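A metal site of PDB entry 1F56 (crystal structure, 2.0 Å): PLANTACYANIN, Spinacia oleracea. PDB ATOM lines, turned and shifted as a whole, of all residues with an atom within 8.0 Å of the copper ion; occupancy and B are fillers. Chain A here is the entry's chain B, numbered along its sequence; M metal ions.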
ATOM      1  N   TRP A   7      24.048 -23.641  16.509  1.00  0.00           N
ATOM      2  CA  TRP A   7      23.514 -22.862  15.393  1.00  0.00           C
ATOM      3  C   TRP A   7      23.226 -21.410  15.768  1.00  0.00           C
ATOM      4  O   TRP A   7      22.239 -21.125  16.426  1.00  0.00           O
ATOM      5  CB  TRP A   7      22.237 -23.574  14.906  1.00  0.00           C
ATOM      6  CG  TRP A   7      21.631 -23.109  13.593  1.00  0.00           C
ATOM      7  CD1 TRP A   7      20.333 -22.744  13.379  1.00  0.00           C
ATOM      8  CD2 TRP A   7      22.274 -23.072  12.296  1.00  0.00           C
ATOM      9  NE1 TRP A   7      20.127 -22.483  12.044  1.00  0.00           N
ATOM     10  CE2 TRP A   7      21.290 -22.674  11.363  1.00  0.00           C
ATOM     11  CE3 TRP A   7      23.576 -23.346  11.848  1.00  0.00           C
ATOM     12  CZ2 TRP A   7      21.563 -22.543   9.991  1.00  0.00           C
ATOM     13  CZ3 TRP A   7      23.855 -23.203  10.469  1.00  0.00           C
ATOM     14  CH2 TRP A   7      22.849 -22.809   9.559  1.00  0.00           C
ATOM     15  N   SER A   8      24.100 -20.493  15.356  1.00  0.00           N
ATOM     16  CA  SER A   8      23.894 -19.063  15.617  1.00  0.00           C
ATOM     17  C   SER A   8      24.646 -18.283  14.556  1.00  0.00           C
ATOM     18  O   SER A   8      25.138 -18.863  13.583  1.00  0.00           O
ATOM     19  CB  SER A   8      24.409 -18.677  17.025  1.00  0.00           C
ATOM     20  OG  SER A   8      23.999 -17.360  17.397  1.00  0.00           O
ATOM     21  N   PHE A   9      24.724 -16.969  14.710  1.00  0.00           N
ATOM     22  CA  PHE A   9      25.449 -16.152  13.744  1.00  0.00           C
ATOM     23  C   PHE A   9      26.879 -16.669  13.626  1.00  0.00           C
ATOM     24  O   PHE A   9      27.453 -16.666  12.546  1.00  0.00           O
ATOM     25  CB  PHE A   9      25.388 -14.697  14.167  1.00  0.00           C
ATOM     26  CG  PHE A   9      24.008 -14.156  14.196  1.00  0.00           C
ATOM     27  CD1 PHE A   9      23.348 -13.860  13.005  1.00  0.00           C
ATOM     28  CD2 PHE A   9      23.345 -13.990  15.397  1.00  0.00           C
ATOM     29  CE1 PHE A   9      22.029 -13.396  13.026  1.00  0.00           C
ATOM     30  CE2 PHE A   9      22.033 -13.532  15.428  1.00  0.00           C
ATOM     31  CZ  PHE A   9      21.373 -13.237  14.238  1.00  0.00           C
ATOM     32  N   TYR A  29      19.568 -24.488  19.040  1.00  0.00           N
ATOM     33  CA  TYR A  29      19.349 -23.050  19.156  1.00  0.00           C
ATOM     34  C   TYR A  29      18.042 -22.885  19.903  1.00  0.00           C
ATOM     35  O   TYR A  29      17.427 -23.885  20.280  1.00  0.00           O
ATOM     36  CB  TYR A  29      19.256 -22.390  17.774  1.00  0.00           C
ATOM     37  CG  TYR A  29      18.222 -23.010  16.864  1.00  0.00           C
ATOM     38  CD1 TYR A  29      18.455 -24.221  16.203  1.00  0.00           C
ATOM     39  CD2 TYR A  29      16.972 -22.402  16.693  1.00  0.00           C
ATOM     40  CE1 TYR A  29      17.473 -24.810  15.397  1.00  0.00           C
ATOM     41  CE2 TYR A  29      15.981 -22.993  15.891  1.00  0.00           C
ATOM     42  CZ  TYR A  29      16.244 -24.193  15.247  1.00  0.00           C
ATOM     43  OH  TYR A  29      15.257 -24.778  14.476  1.00  0.00           O
ATOM     44  N   GLY A  32      12.133 -20.511  17.875  1.00  0.00           N
ATOM     45  CA  GLY A  32      11.592 -19.203  17.553  1.00  0.00           C
ATOM     46  C   GLY A  32      12.600 -18.119  17.199  1.00  0.00           C
ATOM     47  O   GLY A  32      12.220 -17.112  16.620  1.00  0.00           O
ATOM     48  N   GLN A  33      13.862 -18.322  17.522  1.00  0.00           N
ATOM     49  CA  GLN A  33      14.901 -17.317  17.211  1.00  0.00           C
ATOM     50  C   GLN A  33      15.584 -17.540  15.854  1.00  0.00           C
ATOM     51  O   GLN A  33      16.153 -16.614  15.280  1.00  0.00           O
ATOM     52  CB  GLN A  33      15.973 -17.336  18.313  1.00  0.00           C
ATOM     53  CG  GLN A  33      15.453 -16.972  19.708  1.00  0.00           C
ATOM     54  CD  GLN A  33      14.873 -15.574  19.749  1.00  0.00           C
ATOM     55  OE1 GLN A  33      13.763 -15.374  20.215  1.00  0.00           O
ATOM     56  NE2 GLN A  33      15.639 -14.595  19.256  1.00  0.00           N
ATOM     57  N   HIS A  34      15.537 -18.776  15.351  1.00  0.00           N
ATOM     58  CA  HIS A  34      16.158 -19.134  14.076  1.00  0.00           C
ATOM     59  C   HIS A  34      15.393 -20.332  13.502  1.00  0.00           C
ATOM     60  O   HIS A  34      14.459 -20.830  14.109  1.00  0.00           O
ATOM     61  CB  HIS A  34      17.617 -19.609  14.278  1.00  0.00           C
ATOM     62  CG  HIS A  34      18.503 -18.629  14.995  1.00  0.00           C
ATOM     63  ND1 HIS A  34      19.017 -17.502  14.389  1.00  0.00           N
ATOM     64  CD2 HIS A  34      18.970 -18.626  16.262  1.00  0.00           C
ATOM     65  CE1 HIS A  34      19.761 -16.842  15.258  1.00  0.00           C
ATOM     66  NE2 HIS A  34      19.751 -17.494  16.399  1.00  0.00           N
ATOM     67  N   ASN A  35      15.803 -20.766  12.319  1.00  0.00           N
ATOM     68  CA  ASN A  35      15.242 -21.975  11.727  1.00  0.00           C
ATOM     69  C   ASN A  35      16.368 -22.565  10.916  1.00  0.00           C
ATOM     70  O   ASN A  35      17.425 -21.942  10.788  1.00  0.00           O
ATOM     71  CB  ASN A  35      13.985 -21.685  10.868  1.00  0.00           C
ATOM     72  CG  ASN A  35      14.285 -20.916   9.607  1.00  0.00           C
ATOM     73  OD1 ASN A  35      15.438 -20.659   9.285  1.00  0.00           O
ATOM     74  ND2 ASN A  35      13.238 -20.541   8.885  1.00  0.00           N
ATOM     75  N   VAL A  36      16.179 -23.782  10.420  1.00  0.00           N
ATOM     76  CA  VAL A  36      17.190 -24.441   9.605  1.00  0.00           C
ATOM     77  C   VAL A  36      16.484 -24.798   8.306  1.00  0.00           C
ATOM     78  O   VAL A  36      15.488 -25.544   8.324  1.00  0.00           O
ATOM     79  CB  VAL A  36      17.709 -25.758  10.218  1.00  0.00           C
ATOM     80  CG1 VAL A  36      18.806 -26.330   9.301  1.00  0.00           C
ATOM     81  CG2 VAL A  36      18.239 -25.526  11.629  1.00  0.00           C
ATOM     82  N   ILE A  73      20.779 -23.007   5.682  1.00  0.00           N
ATOM     83  CA  ILE A  73      20.834 -21.589   6.025  1.00  0.00           C
ATOM     84  C   ILE A  73      19.679 -21.299   6.949  1.00  0.00           C
ATOM     85  O   ILE A  73      18.752 -22.113   7.080  1.00  0.00           O
ATOM     86  CB  ILE A  73      20.638 -20.635   4.793  1.00  0.00           C
ATOM     87  CG1 ILE A  73      19.186 -20.707   4.287  1.00  0.00           C
ATOM     88  CG2 ILE A  73      21.660 -20.958   3.702  1.00  0.00           C
ATOM     89  CD1 ILE A  73      18.861 -19.637   3.270  1.00  0.00           C
ATOM     90  N   CYS A  74      19.754 -20.157   7.628  1.00  0.00           N
ATOM     91  CA  CYS A  74      18.657 -19.701   8.475  1.00  0.00           C
ATOM     92  C   CYS A  74      17.999 -18.658   7.562  1.00  0.00           C
ATOM     93  O   CYS A  74      18.695 -17.793   7.022  1.00  0.00           O
ATOM     94  CB  CYS A  74      19.159 -19.022   9.735  1.00  0.00           C
ATOM     95  SG  CYS A  74      17.795 -18.309  10.674  1.00  0.00           S
ATOM     96  N   SER A  75      16.694 -18.724   7.384  1.00  0.00           N
ATOM     97  CA  SER A  75      16.060 -17.791   6.467  1.00  0.00           C
ATOM     98  C   SER A  75      15.553 -16.505   7.069  1.00  0.00           C
ATOM     99  O   SER A  75      14.980 -15.694   6.354  1.00  0.00           O
ATOM    100  CB  SER A  75      14.912 -18.458   5.708  1.00  0.00           C
ATOM    101  OG  SER A  75      13.851 -18.810   6.589  1.00  0.00           O
ATOM    102  N   PHE A  76      15.748 -16.297   8.376  1.00  0.00           N
ATOM    103  CA  PHE A  76      15.238 -15.074   8.986  1.00  0.00           C
ATOM    104  C   PHE A  76      15.987 -13.872   8.391  1.00  0.00           C
ATOM    105  O   PHE A  76      17.151 -13.975   8.042  1.00  0.00           O
ATOM    106  CB  PHE A  76      15.371 -15.120  10.513  1.00  0.00           C
ATOM    107  CG  PHE A  76      14.392 -16.068  11.182  1.00  0.00           C
ATOM    108  CD1 PHE A  76      13.593 -16.940  10.436  1.00  0.00           C
ATOM    109  CD2 PHE A  76      14.315 -16.135  12.577  1.00  0.00           C
ATOM    110  CE1 PHE A  76      12.744 -17.863  11.057  1.00  0.00           C
ATOM    111  CE2 PHE A  76      13.475 -17.053  13.215  1.00  0.00           C
ATOM    112  CZ  PHE A  76      12.693 -17.921  12.459  1.00  0.00           C
ATOM    113  N   PRO A  77      15.306 -12.721   8.253  1.00  0.00           N
ATOM    114  CA  PRO A  77      15.901 -11.500   7.683  1.00  0.00           C
ATOM    115  C   PRO A  77      17.317 -11.180   8.146  1.00  0.00           C
ATOM    116  O   PRO A  77      17.559 -10.902   9.317  1.00  0.00           O
ATOM    117  CB  PRO A  77      14.909 -10.406   8.073  1.00  0.00           C
ATOM    118  CG  PRO A  77      13.614 -11.138   8.108  1.00  0.00           C
ATOM    119  CD  PRO A  77      13.981 -12.417   8.819  1.00  0.00           C
ATOM    120  N   GLY A  78      18.241 -11.231   7.185  1.00  0.00           N
ATOM    121  CA  GLY A  78      19.629 -10.935   7.463  1.00  0.00           C
ATOM    122  C   GLY A  78      20.422 -12.003   8.189  1.00  0.00           C
ATOM    123  O   GLY A  78      21.625 -11.822   8.361  1.00  0.00           O
ATOM    124  N   HIS A  79      19.810 -13.112   8.609  1.00  0.00           N
ATOM    125  CA  HIS A  79      20.603 -14.118   9.318  1.00  0.00           C
ATOM    126  C   HIS A  79      21.600 -14.864   8.443  1.00  0.00           C
ATOM    127  O   HIS A  79      22.766 -15.046   8.831  1.00  0.00           O
ATOM    128  CB  HIS A  79      19.680 -15.103  10.051  1.00  0.00           C
ATOM    129  CG  HIS A  79      18.979 -14.486  11.231  1.00  0.00           C
ATOM    130  ND1 HIS A  79      18.498 -15.235  12.287  1.00  0.00           N
ATOM    131  CD2 HIS A  79      18.690 -13.196  11.516  1.00  0.00           C
ATOM    132  CE1 HIS A  79      17.943 -14.432  13.181  1.00  0.00           C
ATOM    133  NE2 HIS A  79      18.041 -13.192  12.735  1.00  0.00           N
ATOM    134  N   CYS A  80      21.194 -15.281   7.255  1.00  0.00           N
ATOM    135  CA  CYS A  80      22.123 -15.985   6.379  1.00  0.00           C
ATOM    136  C   CYS A  80      23.249 -15.015   6.000  1.00  0.00           C
ATOM    137  O   CYS A  80      24.420 -15.410   5.975  1.00  0.00           O
ATOM    138  CB  CYS A  80      21.392 -16.479   5.144  1.00  0.00           C
ATOM    139  SG  CYS A  80      22.399 -17.326   3.890  1.00  0.00           S
ATOM    140  N   MET A  84      24.846 -17.251   9.174  1.00  0.00           N
ATOM    141  CA  MET A  84      24.124 -18.502   9.423  1.00  0.00           C
ATOM    142  C   MET A  84      23.902 -19.323   8.182  1.00  0.00           C
ATOM    143  O   MET A  84      22.815 -19.305   7.572  1.00  0.00           O
ATOM    144  CB  MET A  84      22.792 -18.215  10.113  1.00  0.00           C
ATOM    145  CG  MET A  84      22.957 -17.527  11.445  1.00  0.00           C
ATOM    146  SD  MET A  84      21.487 -17.673  12.457  1.00  0.00           S
ATOM    147  CE  MET A  84      21.578 -19.429  12.936  1.00  0.00           C
HETATM  148 CU    CU M   1      18.741 -17.224  12.333  1.00  0.00          CU
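SG of Cys 74 lies close to N of Phe 76. SG of Cys 74 sits close to N of Asn 35, at 3.6 Å.
Gln 33 touches the copper ion. Of the 18 residues printed, 5 come within 4 Å of the copper ion.
ND1 of His 79 is bound to the copper ion, 2.0 Å away. A ring nitrogen (ND1) of His 34 is bound to the copper ion (2.1 Å). SG of Cys 74 is bound to the copper ion (2.2 Å). The side-chain sulfur (SD) of Met 84 binds the copper ion. The copper ion has four donor atoms within binding distance.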
